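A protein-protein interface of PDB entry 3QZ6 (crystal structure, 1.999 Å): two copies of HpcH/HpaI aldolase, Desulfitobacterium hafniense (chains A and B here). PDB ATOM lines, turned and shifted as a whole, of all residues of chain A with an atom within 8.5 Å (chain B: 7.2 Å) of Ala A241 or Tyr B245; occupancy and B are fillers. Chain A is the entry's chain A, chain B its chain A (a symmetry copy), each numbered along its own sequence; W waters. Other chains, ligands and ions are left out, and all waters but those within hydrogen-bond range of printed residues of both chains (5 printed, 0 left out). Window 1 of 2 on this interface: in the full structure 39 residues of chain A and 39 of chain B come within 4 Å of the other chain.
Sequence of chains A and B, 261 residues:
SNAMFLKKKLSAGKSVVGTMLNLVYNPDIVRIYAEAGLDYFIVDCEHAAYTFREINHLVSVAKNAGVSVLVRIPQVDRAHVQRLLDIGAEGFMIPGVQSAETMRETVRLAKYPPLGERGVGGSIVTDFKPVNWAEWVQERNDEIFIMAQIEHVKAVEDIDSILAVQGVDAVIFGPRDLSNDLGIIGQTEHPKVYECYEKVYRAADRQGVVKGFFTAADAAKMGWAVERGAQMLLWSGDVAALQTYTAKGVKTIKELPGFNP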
ATOM      1  N   THR A  19       6.065   9.196  -7.060  1.00  0.00           N
ATOM      2  CA  THR A  19       7.324   9.178  -6.341  1.00  0.00           C
ATOM      3  C   THR A  19       8.408   8.627  -7.262  1.00  0.00           C
ATOM      4  O   THR A  19       8.101   8.035  -8.304  1.00  0.00           O
ATOM      5  CB  THR A  19       7.196   8.349  -5.044  1.00  0.00           C
ATOM      6  OG1 THR A  19       8.219   8.728  -4.123  1.00  0.00           O
ATOM      7  CG2 THR A  19       7.285   6.843  -5.336  1.00  0.00           C
ATOM      8  N   MET A  20       9.674   8.831  -6.899  1.00  0.00           N
ATOM      9  CA  MET A  20      10.785   8.293  -7.677  1.00  0.00           C
ATOM     10  C   MET A  20      11.073   6.841  -7.270  1.00  0.00           C
ATOM     11  O   MET A  20      10.915   6.478  -6.104  1.00  0.00           O
ATOM     12  CB  MET A  20      12.051   9.125  -7.452  1.00  0.00           C
ATOM     13  CG  MET A  20      11.967  10.579  -7.924  1.00  0.00           C
ATOM     14  SD  MET A  20      11.773  10.667  -9.851  1.00  0.00           S
ATOM     15  CE  MET A  20      13.277   9.496 -10.365  1.00  0.00           C
ATOM     16  N   VAL A  24      14.372  -0.201  -5.530  1.00  0.00           N
ATOM     17  CA  VAL A  24      13.589  -1.438  -5.536  1.00  0.00           C
ATOM     18  C   VAL A  24      13.272  -1.869  -6.967  1.00  0.00           C
ATOM     19  O   VAL A  24      12.881  -1.034  -7.796  1.00  0.00           O
ATOM     20  CB  VAL A  24      12.295  -1.274  -4.710  1.00  0.00           C
ATOM     21  CG1 VAL A  24      11.481  -2.597  -4.696  1.00  0.00           C
ATOM     22  CG2 VAL A  24      12.641  -0.827  -3.271  1.00  0.00           C
ATOM     23  N   ILE A  29       6.594  -3.756  -5.423  1.00  0.00           N
ATOM     24  CA  ILE A  29       6.641  -2.346  -5.038  1.00  0.00           C
ATOM     25  C   ILE A  29       5.444  -1.626  -5.668  1.00  0.00           C
ATOM     26  O   ILE A  29       4.936  -0.645  -5.125  1.00  0.00           O
ATOM     27  CB  ILE A  29       7.949  -1.640  -5.473  1.00  0.00           C
ATOM     28  CG1 ILE A  29       8.060  -0.255  -4.820  1.00  0.00           C
ATOM     29  CG2 ILE A  29       8.036  -1.496  -7.016  1.00  0.00           C
ATOM     30  CD1 ILE A  29       8.058  -0.305  -3.305  1.00  0.00           C
ATOM     31  N   TYR A  33       2.750   0.637  -3.733  1.00  0.00           N
ATOM     32  CA  TYR A  33       2.493   2.016  -4.133  1.00  0.00           C
ATOM     33  C   TYR A  33       1.009   2.273  -4.439  1.00  0.00           C
ATOM     34  O   TYR A  33       0.472   3.336  -4.121  1.00  0.00           O
ATOM     35  CB  TYR A  33       3.397   2.417  -5.312  1.00  0.00           C
ATOM     36  CG  TYR A  33       4.819   2.805  -4.891  1.00  0.00           C
ATOM     37  CD1 TYR A  33       5.155   2.959  -3.546  1.00  0.00           C
ATOM     38  CD2 TYR A  33       5.806   3.042  -5.838  1.00  0.00           C
ATOM     39  CE1 TYR A  33       6.450   3.337  -3.158  1.00  0.00           C
ATOM     40  CE2 TYR A  33       7.099   3.409  -5.468  1.00  0.00           C
ATOM     41  CZ  TYR A  33       7.415   3.562  -4.131  1.00  0.00           C
ATOM     42  OH  TYR A  33       8.703   3.941  -3.773  1.00  0.00           O
ATOM     43  N   ALA A  36      -0.688   2.570  -1.156  1.00  0.00           N
ATOM     44  CA  ALA A  36      -0.346   3.841  -0.514  1.00  0.00           C
ATOM     45  C   ALA A  36      -1.036   5.041  -1.157  1.00  0.00           C
ATOM     46  O   ALA A  36      -0.922   6.163  -0.663  1.00  0.00           O
ATOM     47  CB  ALA A  36       1.158   4.052  -0.499  1.00  0.00           C
ATOM     48  N   THR A 215       9.540  17.641  -4.760  1.00  0.00           N
ATOM     49  CA  THR A 215      10.151  17.934  -3.473  1.00  0.00           C
ATOM     50  C   THR A 215      10.764  16.659  -2.901  1.00  0.00           C
ATOM     51  O   THR A 215      10.150  15.587  -2.927  1.00  0.00           O
ATOM     52  CB  THR A 215       9.174  18.625  -2.505  1.00  0.00           C
ATOM     53  OG1 THR A 215       9.904  19.139  -1.386  1.00  0.00           O
ATOM     54  CG2 THR A 215       8.109  17.661  -2.031  1.00  0.00           C
ATOM     55  N   ALA A 216      11.998  16.776  -2.427  1.00  0.00           N
ATOM     56  CA  ALA A 216      12.837  15.608  -2.174  1.00  0.00           C
ATOM     57  C   ALA A 216      12.604  14.964  -0.824  1.00  0.00           C
ATOM     58  O   ALA A 216      12.827  13.760  -0.655  1.00  0.00           O
ATOM     59  CB  ALA A 216      14.313  15.969  -2.333  1.00  0.00           C
ATOM     60  N   ALA A 217      12.168  15.760   0.143  1.00  0.00           N
ATOM     61  CA  ALA A 217      12.066  15.266   1.507  1.00  0.00           C
ATOM     62  C   ALA A 217      10.713  15.508   2.182  1.00  0.00           C
ATOM     63  O   ALA A 217      10.022  14.545   2.543  1.00  0.00           O
ATOM     64  CB  ALA A 217      13.198  15.836   2.360  1.00  0.00           C
ATOM     65  N   ASP A 218      10.341  16.776   2.365  1.00  0.00           N
ATOM     66  CA  ASP A 218       9.194  17.099   3.222  1.00  0.00           C
ATOM     67  C   ASP A 218       7.888  17.325   2.463  1.00  0.00           C
ATOM     68  O   ASP A 218       7.717  18.334   1.787  1.00  0.00           O
ATOM     69  CB  ASP A 218       9.495  18.291   4.132  1.00  0.00           C
ATOM     70  CG  ASP A 218       8.376  18.556   5.139  1.00  0.00           C
ATOM     71  OD1 ASP A 218       7.527  17.659   5.356  1.00  0.00           O
ATOM     72  OD2 ASP A 218       8.352  19.664   5.721  1.00  0.00           O
ATOM     73  N   ALA A 219       6.963  16.380   2.606  1.00  0.00           N
ATOM     74  CA  ALA A 219       5.717  16.395   1.854  1.00  0.00           C
ATOM     75  C   ALA A 219       4.987  17.739   1.962  1.00  0.00           C
ATOM     76  O   ALA A 219       4.364  18.196   1.001  1.00  0.00           O
ATOM     77  CB  ALA A 219       4.818  15.259   2.306  1.00  0.00           C
ATOM     78  N   TRP A 235       6.883  13.430  -5.143  1.00  0.00           N
ATOM     79  CA  TRP A 235       7.420  13.554  -3.786  1.00  0.00           C
ATOM     80  C   TRP A 235       8.356  12.411  -3.420  1.00  0.00           C
ATOM     81  O   TRP A 235       7.976  11.239  -3.474  1.00  0.00           O
ATOM     82  CB  TRP A 235       6.280  13.637  -2.757  1.00  0.00           C
ATOM     83  CG  TRP A 235       6.763  13.435  -1.349  1.00  0.00           C
ATOM     84  CD1 TRP A 235       7.520  14.300  -0.609  1.00  0.00           C
ATOM     85  CD2 TRP A 235       6.539  12.290  -0.522  1.00  0.00           C
ATOM     86  NE1 TRP A 235       7.787  13.754   0.625  1.00  0.00           N
ATOM     87  CE2 TRP A 235       7.193  12.523   0.702  1.00  0.00           C
ATOM     88  CE3 TRP A 235       5.850  11.090  -0.697  1.00  0.00           C
ATOM     89  CZ2 TRP A 235       7.181  11.596   1.738  1.00  0.00           C
ATOM     90  CZ3 TRP A 235       5.841  10.174   0.340  1.00  0.00           C
ATOM     91  CH2 TRP A 235       6.492  10.436   1.538  1.00  0.00           C
ATOM     92  N   SER A 236       9.584  12.762  -3.059  1.00  0.00           N
ATOM     93  CA  SER A 236      10.534  11.808  -2.477  1.00  0.00           C
ATOM     94  C   SER A 236      10.775  10.574  -3.354  1.00  0.00           C
ATOM     95  O   SER A 236      10.794  10.664  -4.588  1.00  0.00           O
ATOM     96  CB  SER A 236      10.071  11.401  -1.067  1.00  0.00           C
ATOM     97  OG  SER A 236      11.093  10.701  -0.372  1.00  0.00           O
ATOM     98  N   GLY A 237      10.962   9.417  -2.727  1.00  0.00           N
ATOM     99  CA  GLY A 237      11.274   8.214  -3.487  1.00  0.00           C
ATOM    100  C   GLY A 237      11.538   7.031  -2.575  1.00  0.00           C
ATOM    101  O   GLY A 237      11.632   7.201  -1.361  1.00  0.00           O
ATOM    102  N   ASP A 238      11.675   5.840  -3.152  1.00  0.00           N
ATOM    103  CA  ASP A 238      11.840   4.631  -2.352  1.00  0.00           C
ATOM    104  C   ASP A 238      13.089   4.676  -1.475  1.00  0.00           C
ATOM    105  O   ASP A 238      13.055   4.284  -0.307  1.00  0.00           O
ATOM    106  CB  ASP A 238      11.853   3.375  -3.243  1.00  0.00           C
ATOM    107  CG  ASP A 238      12.980   3.393  -4.271  1.00  0.00           C
ATOM    108  OD1 ASP A 238      13.417   4.495  -4.689  1.00  0.00           O
ATOM    109  OD2 ASP A 238      13.428   2.300  -4.670  1.00  0.00           O
ATOM    110  N   VAL A 239      14.195   5.139  -2.035  1.00  0.00           N
ATOM    111  CA  VAL A 239      15.429   5.218  -1.259  1.00  0.00           C
ATOM    112  C   VAL A 239      15.280   6.132  -0.039  1.00  0.00           C
ATOM    113  O   VAL A 239      15.660   5.757   1.064  1.00  0.00           O
ATOM    114  CB  VAL A 239      16.618   5.695  -2.124  1.00  0.00           C
ATOM    115  CG1 VAL A 239      17.840   5.917  -1.252  1.00  0.00           C
ATOM    116  CG2 VAL A 239      16.928   4.654  -3.218  1.00  0.00           C
ATOM    117  N   ALA A 240      14.744   7.333  -0.233  1.00  0.00           N
ATOM    118  CA  ALA A 240      14.564   8.251   0.900  1.00  0.00           C
ATOM    119  C   ALA A 240      13.627   7.641   1.937  1.00  0.00           C
ATOM    120  O   ALA A 240      13.836   7.787   3.134  1.00  0.00           O
ATOM    121  CB  ALA A 240      14.031   9.608   0.430  1.00  0.00           C
ATOM    122  N   ALA A 241      12.597   6.946   1.466  1.00  0.00           N
ATOM    123  CA  ALA A 241      11.672   6.270   2.361  1.00  0.00           C
ATOM    124  C   ALA A 241      12.422   5.280   3.247  1.00  0.00           C
ATOM    125  O   ALA A 241      12.285   5.298   4.468  1.00  0.00           O
ATOM    126  CB  ALA A 241      10.565   5.550   1.553  1.00  0.00           C
ATOM    127  N   LEU A 242      13.222   4.417   2.629  1.00  0.00           N
ATOM    128  CA  LEU A 242      13.965   3.412   3.379  1.00  0.00           C
ATOM    129  C   LEU A 242      15.002   4.041   4.309  1.00  0.00           C
ATOM    130  O   LEU A 242      15.146   3.622   5.459  1.00  0.00           O
ATOM    131  CB  LEU A 242      14.614   2.405   2.415  1.00  0.00           C
ATOM    132  CG  LEU A 242      13.607   1.444   1.763  1.00  0.00           C
ATOM    133  CD1 LEU A 242      14.138   0.825   0.450  1.00  0.00           C
ATOM    134  CD2 LEU A 242      13.213   0.346   2.755  1.00  0.00           C
ATOM    135  N   GLN A 243      15.720   5.056   3.836  1.00  0.00           N
ATOM    136  CA  GLN A 243      16.780   5.638   4.665  1.00  0.00           C
ATOM    137  C   GLN A 243      16.206   6.443   5.826  1.00  0.00           C
ATOM    138  O   GLN A 243      16.689   6.361   6.951  1.00  0.00           O
ATOM    139  CB  GLN A 243      17.715   6.522   3.833  1.00  0.00           C
ATOM    140  CG  GLN A 243      18.482   5.748   2.775  1.00  0.00           C
ATOM    141  CD  GLN A 243      19.721   6.482   2.312  1.00  0.00           C
ATOM    142  OE1 GLN A 243      19.642   7.401   1.495  1.00  0.00           O
ATOM    143  NE2 GLN A 243      20.873   6.087   2.842  1.00  0.00           N
ATOM    144  N   THR A 244      15.177   7.226   5.542  1.00  0.00           N
ATOM    145  CA  THR A 244      14.609   8.112   6.546  1.00  0.00           C
ATOM    146  C   THR A 244      13.872   7.333   7.638  1.00  0.00           C
ATOM    147  O   THR A 244      14.170   7.485   8.820  1.00  0.00           O
ATOM    148  CB  THR A 244      13.682   9.145   5.906  1.00  0.00           C
ATOM    149  OG1 THR A 244      14.402   9.837   4.880  1.00  0.00           O
ATOM    150  CG2 THR A 244      13.194  10.158   6.952  1.00  0.00           C
ATOM    151  N   TYR A 245      12.921   6.496   7.242  1.00  0.00           N
ATOM    152  CA  TYR A 245      12.186   5.670   8.198  1.00  0.00           C
ATOM    153  C   TYR A 245      13.127   4.794   9.015  1.00  0.00           C
ATOM    154  O   TYR A 245      13.046   4.770  10.240  1.00  0.00           O
ATOM    155  CB  TYR A 245      11.154   4.801   7.472  1.00  0.00           C
ATOM    156  CG  TYR A 245      10.385   3.826   8.356  1.00  0.00           C
ATOM    157  CD1 TYR A 245       9.143   4.164   8.900  1.00  0.00           C
ATOM    158  CD2 TYR A 245      10.900   2.574   8.641  1.00  0.00           C
ATOM    159  CE1 TYR A 245       8.430   3.256   9.707  1.00  0.00           C
ATOM    160  CE2 TYR A 245      10.203   1.663   9.424  1.00  0.00           C
ATOM    161  CZ  TYR A 245       8.972   2.007   9.958  1.00  0.00           C
ATOM    162  OH  TYR A 245       8.297   1.081  10.740  1.00  0.00           O
ATOM    163  N   THR A 246      14.018   4.063   8.352  1.00  0.00           N
ATOM    164  CA  THR A 246      14.870   3.125   9.087  1.00  0.00           C
ATOM    165  C   THR A 246      15.799   3.846  10.069  1.00  0.00           C
ATOM    166  O   THR A 246      15.925   3.442  11.224  1.00  0.00           O
ATOM    167  CB  THR A 246      15.700   2.217   8.153  1.00  0.00           C
ATOM    168  OG1 THR A 246      14.851   1.665   7.143  1.00  0.00           O
ATOM    169  CG2 THR A 246      16.316   1.057   8.941  1.00  0.00           C
ATOM    170  N   ALA A 247      16.446   4.915   9.617  1.00  0.00           N
ATOM    171  CA  ALA A 247      17.404   5.618  10.463  1.00  0.00           C
ATOM    172  C   ALA A 247      16.724   6.183  11.710  1.00  0.00           C
ATOM    173  O   ALA A 247      17.282   6.132  12.803  1.00  0.00           O
ATOM    174  CB  ALA A 247      18.113   6.730   9.685  1.00  0.00           C
ATOM    175  N   LYS A 248      15.518   6.715  11.537  1.00  0.00           N
ATOM    176  CA  LYS A 248      14.762   7.307  12.638  1.00  0.00           C
ATOM    177  C   LYS A 248      14.484   6.301  13.765  1.00  0.00           C
ATOM    178  O   LYS A 248      14.756   6.565  14.942  1.00  0.00           O
ATOM    179  CB  LYS A 248      13.454   7.896  12.109  1.00  0.00           C
ATOM    180  CG  LYS A 248      12.657   8.696  13.136  1.00  0.00           C
ATOM    181  CD  LYS A 248      11.363   9.224  12.523  1.00  0.00           C
ATOM    182  CE  LYS A 248      10.438   9.810  13.578  1.00  0.00           C
ATOM    183  NZ  LYS A 248      11.062  10.981  14.251  1.00  0.00           N
ATOM    184  N   VAL B 239       9.155  -3.646   4.389  1.00  0.00           N
ATOM    185  CA  VAL B 239       7.788  -3.416   3.931  1.00  0.00           C
ATOM    186  C   VAL B 239       7.081  -2.340   4.761  1.00  0.00           C
ATOM    187  O   VAL B 239       6.473  -1.433   4.206  1.00  0.00           O
ATOM    188  CB  VAL B 239       6.954  -4.716   3.947  1.00  0.00           C
ATOM    189  CG1 VAL B 239       5.503  -4.409   3.621  1.00  0.00           C
ATOM    190  CG2 VAL B 239       7.525  -5.725   2.931  1.00  0.00           C
ATOM    191  N   ALA B 240       7.146  -2.444   6.085  1.00  0.00           N
ATOM    192  CA  ALA B 240       6.498  -1.437   6.936  1.00  0.00           C
ATOM    193  C   ALA B 240       7.105  -0.060   6.689  1.00  0.00           C
ATOM    194  O   ALA B 240       6.402   0.941   6.674  1.00  0.00           O
ATOM    195  CB  ALA B 240       6.609  -1.814   8.417  1.00  0.00           C
ATOM    196  N   ALA B 241       8.417  -0.022   6.483  1.00  0.00           N
ATOM    197  CA  ALA B 241       9.095   1.228   6.179  1.00  0.00           C
ATOM    198  C   ALA B 241       8.499   1.862   4.927  1.00  0.00           C
ATOM    199  O   ALA B 241       8.124   3.032   4.930  1.00  0.00           O
ATOM    200  CB  ALA B 241      10.615   0.989   6.000  1.00  0.00           C
ATOM    201  N   LEU B 242       8.405   1.084   3.853  1.00  0.00           N
ATOM    202  CA  LEU B 242       7.873   1.597   2.598  1.00  0.00           C
ATOM    203  C   LEU B 242       6.399   1.984   2.713  1.00  0.00           C
ATOM    204  O   LEU B 242       5.985   3.030   2.209  1.00  0.00           O
ATOM    205  CB  LEU B 242       8.097   0.574   1.470  1.00  0.00           C
ATOM    206  CG  LEU B 242       9.562   0.468   1.022  1.00  0.00           C
ATOM    207  CD1 LEU B 242       9.874  -0.872   0.317  1.00  0.00           C
ATOM    208  CD2 LEU B 242       9.922   1.649   0.116  1.00  0.00           C
ATOM    209  N   GLN B 243       5.597   1.164   3.388  1.00  0.00           N
ATOM    210  CA  GLN B 243       4.162   1.454   3.458  1.00  0.00           C
ATOM    211  C   GLN B 243       3.875   2.651   4.359  1.00  0.00           C
ATOM    212  O   GLN B 243       3.059   3.507   4.031  1.00  0.00           O
ATOM    213  CB  GLN B 243       3.371   0.236   3.945  1.00  0.00           C
ATOM    214  CG  GLN B 243       3.444  -0.943   2.991  1.00  0.00           C
ATOM    215  CD  GLN B 243       2.311  -1.922   3.201  1.00  0.00           C
ATOM    216  OE1 GLN B 243       2.347  -2.743   4.119  1.00  0.00           O
ATOM    217  NE2 GLN B 243       1.290  -1.835   2.355  1.00  0.00           N
ATOM    218  N   THR B 244       4.547   2.699   5.499  1.00  0.00           N
ATOM    219  CA  THR B 244       4.286   3.740   6.480  1.00  0.00           C
ATOM    220  C   THR B 244       4.769   5.109   5.996  1.00  0.00           C
ATOM    221  O   THR B 244       3.996   6.062   5.953  1.00  0.00           O
ATOM    222  CB  THR B 244       4.917   3.395   7.829  1.00  0.00           C
ATOM    223  OG1 THR B 244       4.455   2.102   8.235  1.00  0.00           O
ATOM    224  CG2 THR B 244       4.524   4.430   8.893  1.00  0.00           C
ATOM    225  N   TYR B 245       6.039   5.202   5.626  1.00  0.00           N
ATOM    226  CA  TYR B 245       6.593   6.452   5.105  1.00  0.00           C
ATOM    227  C   TYR B 245       5.821   6.936   3.886  1.00  0.00           C
ATOM    228  O   TYR B 245       5.413   8.093   3.828  1.00  0.00           O
ATOM    229  CB  TYR B 245       8.074   6.275   4.755  1.00  0.00           C
ATOM    230  CG  TYR B 245       8.740   7.488   4.116  1.00  0.00           C
ATOM    231  CD1 TYR B 245       9.434   8.425   4.885  1.00  0.00           C
ATOM    232  CD2 TYR B 245       8.677   7.689   2.748  1.00  0.00           C
ATOM    233  CE1 TYR B 245      10.059   9.538   4.290  1.00  0.00           C
ATOM    234  CE2 TYR B 245       9.300   8.775   2.144  1.00  0.00           C
ATOM    235  CZ  TYR B 245       9.987   9.697   2.916  1.00  0.00           C
ATOM    236  OH  TYR B 245      10.595  10.775   2.290  1.00  0.00           O
ATOM    237  N   THR B 246       5.618   6.067   2.900  1.00  0.00           N
ATOM    238  CA  THR B 246       4.975   6.518   1.663  1.00  0.00           C
ATOM    239  C   THR B 246       3.535   6.984   1.903  1.00  0.00           C
ATOM    240  O   THR B 246       3.129   8.039   1.420  1.00  0.00           O
ATOM    241  CB  THR B 246       4.997   5.443   0.554  1.00  0.00           C
ATOM    242  OG1 THR B 246       6.317   4.902   0.438  1.00  0.00           O
ATOM    243  CG2 THR B 246       4.616   6.057  -0.796  1.00  0.00           C
ATOM    244  N   ALA B 247       2.764   6.204   2.654  1.00  0.00           N
ATOM    245  CA  ALA B 247       1.360   6.536   2.875  1.00  0.00           C
ATOM    246  C   ALA B 247       1.221   7.878   3.592  1.00  0.00           C
ATOM    247  O   ALA B 247       0.343   8.672   3.265  1.00  0.00           O
ATOM    248  CB  ALA B 247       0.649   5.429   3.657  1.00  0.00           C
ATOM    249  N   LYS B 248       2.093   8.122   4.565  1.00  0.00           N
ATOM    250  CA  LYS B 248       2.062   9.358   5.346  1.00  0.00           C
ATOM    251  C   LYS B 248       2.235  10.608   4.471  1.00  0.00           C
ATOM    252  O   LYS B 248       1.443  11.555   4.542  1.00  0.00           O
ATOM    253  CB  LYS B 248       3.138   9.308   6.431  1.00  0.00           C
ATOM    254  CG  LYS B 248       3.092  10.468   7.424  1.00  0.00           C
ATOM    255  CD  LYS B 248       4.213  10.343   8.452  1.00  0.00           C
ATOM    256  CE  LYS B 248       4.345  11.600   9.296  1.00  0.00           C
ATOM    257  NZ  LYS B 248       3.110  11.851  10.087  1.00  0.00           N
ATOM    258  N   GLY B 249       3.262  10.604   3.631  1.00  0.00           N
ATOM    259  CA  GLY B 249       3.521  11.734   2.757  1.00  0.00           C
ATOM    260  C   GLY B 249       2.410  11.959   1.755  1.00  0.00           C
ATOM    261  O   GLY B 249       1.968  13.089   1.535  1.00  0.00           O
ATOM    262  N   VAL B 250       1.953  10.876   1.141  1.00  0.00           N
ATOM    263  CA  VAL B 250       0.864  10.958   0.178  1.00  0.00           C
ATOM    264  C   VAL B 250      -0.376  11.578   0.826  1.00  0.00           C
ATOM    265  O   VAL B 250      -1.025  12.445   0.249  1.00  0.00           O
ATOM    266  CB  VAL B 250       0.517   9.573  -0.388  1.00  0.00           C
ATOM    267  CG1 VAL B 250      -0.794   9.622  -1.160  1.00  0.00           C
ATOM    268  CG2 VAL B 250       1.645   9.078  -1.264  1.00  0.00           C
ATOM    269  N   LYS B 251      -0.688  11.142   2.039  1.00  0.00           N
ATOM    270  CA  LYS B 251      -1.860  11.644   2.742  1.00  0.00           C
ATOM    271  C   LYS B 251      -1.717  13.140   3.038  1.00  0.00           C
ATOM    272  O   LYS B 251      -2.657  13.913   2.861  1.00  0.00           O
ATOM    273  CB  LYS B 251      -2.064  10.847   4.028  1.00  0.00           C
ATOM    274  CG  LYS B 251      -3.263  11.246   4.874  1.00  0.00           C
ATOM    275  CD  LYS B 251      -3.412  10.255   6.032  1.00  0.00           C
ATOM    276  CE  LYS B 251      -4.238  10.818   7.183  1.00  0.00           C
ATOM    277  NZ  LYS B 251      -5.671  10.856   6.830  1.00  0.00           N
HETATM  278  O   HOH W   1       1.383   0.557   0.758  1.00  0.00           O
HETATM  279  O   HOH W   2       5.288   1.278  10.941  1.00  0.00           O
HETATM  280  O   HOH W   3      -1.852   7.585   1.785  1.00  0.00           O
HETATM  281  O   HOH W   4      12.954  12.090   3.647  1.00  0.00           O
HETATM  282  O   HOH W   5       8.508   5.253  -1.272  1.00  0.00           O
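Among the printed residues, merely in contact across the chains: Tyr A33 with Thr B246 (3.9 Å), Ala A36 with Val B250 (3.5 Å), Ala A217 with Tyr B245 (3.8 Å), Ala A219 with Gly B249 (3.7 Å), Trp A235 with Tyr B245 (3.3 Å), Trp A235 with Thr B246 (3.6 Å), Trp A235 with Gly B249 (3.5 Å), Ala A241 with Tyr B245 (3.1 Å), Thr A244 with Tyr B245 (3.99 Å), Tyr A245 with Ala B241 (3.1 Å) and Tyr A245 with Thr B244 (3.99 Å).
Water W5 bridges OG1 of Thr B246 (2.8 Å) and OH of Tyr A33 (2.8 Å).
Water W3 lies within hydrogen-bond range of the backbone carbonyl oxygen of Ala B247 (2.9 Å) and the backbone carbonyl oxygen of Ala A36 (3.0 Å).
Water W1 lies within hydrogen-bond range of NE2 of Gln B243 and N of Ala A36.
Water W4 lies within hydrogen-bond range of the side-chain hydroxyl of Thr A244 (2.9 Å) and the side-chain hydroxyl of Tyr B245 (3.0 Å).
Water W2 bridges OG1 of Thr B244 and OH of Tyr A245.
Hydrophobic or aromatic side chains of chain B within 4 Å of the printed part of chain A: Ala B241, Tyr B245 and Val B250.
Hydrophobic or aromatic side chains of chain A within 4 Å of the printed part of chain B: Tyr A33, Ala A219, Trp A235, Ala A241 and Tyr A245.
Of the printed residues of chain B, Ala A217 touches Tyr B245 (3.8 Å).
Of the printed residues of chain B, Ala A219 touches Gly B249.
Printed residues of chain B within 4 Å of Trp A235: Tyr B245 (3.3 Å), Thr B246 (3.6 Å) and Gly B249 (3.5 Å).
The nearest residue of chain B that does not touch Ala A241 is Leu B242 (4.2 Å).
Ala A241 touches Tyr B245, and with the chains exchanged Tyr A245 touches Ala B241.
Thr A244 touches Tyr B245, and with the chains exchanged Tyr A245 touches Thr B244.
O of Ser A236 sits close to OG1 of Thr A19.
The backbone carbonyl oxygen (O) of Ser A236 lies within hydrogen-bond range of the backbone NH (N) of Met A20.
N of Ser A236 is in hydrogen-bond range of O of Thr A215, at 2.9 Å.
The backbone carbonyl oxygen (O) of Ala A217 lies within hydrogen-bond range of the indole nitrogen (NE1) of Trp A235.
The side-chain hydroxyl of Thr B244 sits at hydrogen-bond distance from the backbone carbonyl oxygen of Ala B240 (2.8 Å).
The backbone carbonyl oxygen of Leu B242 sits at hydrogen-bond distance from the side-chain hydroxyl of Thr B246 (2.6 Å).
OH of Tyr B245 is in hydrogen-bond range of OG of Ser A236 (2.7 Å).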
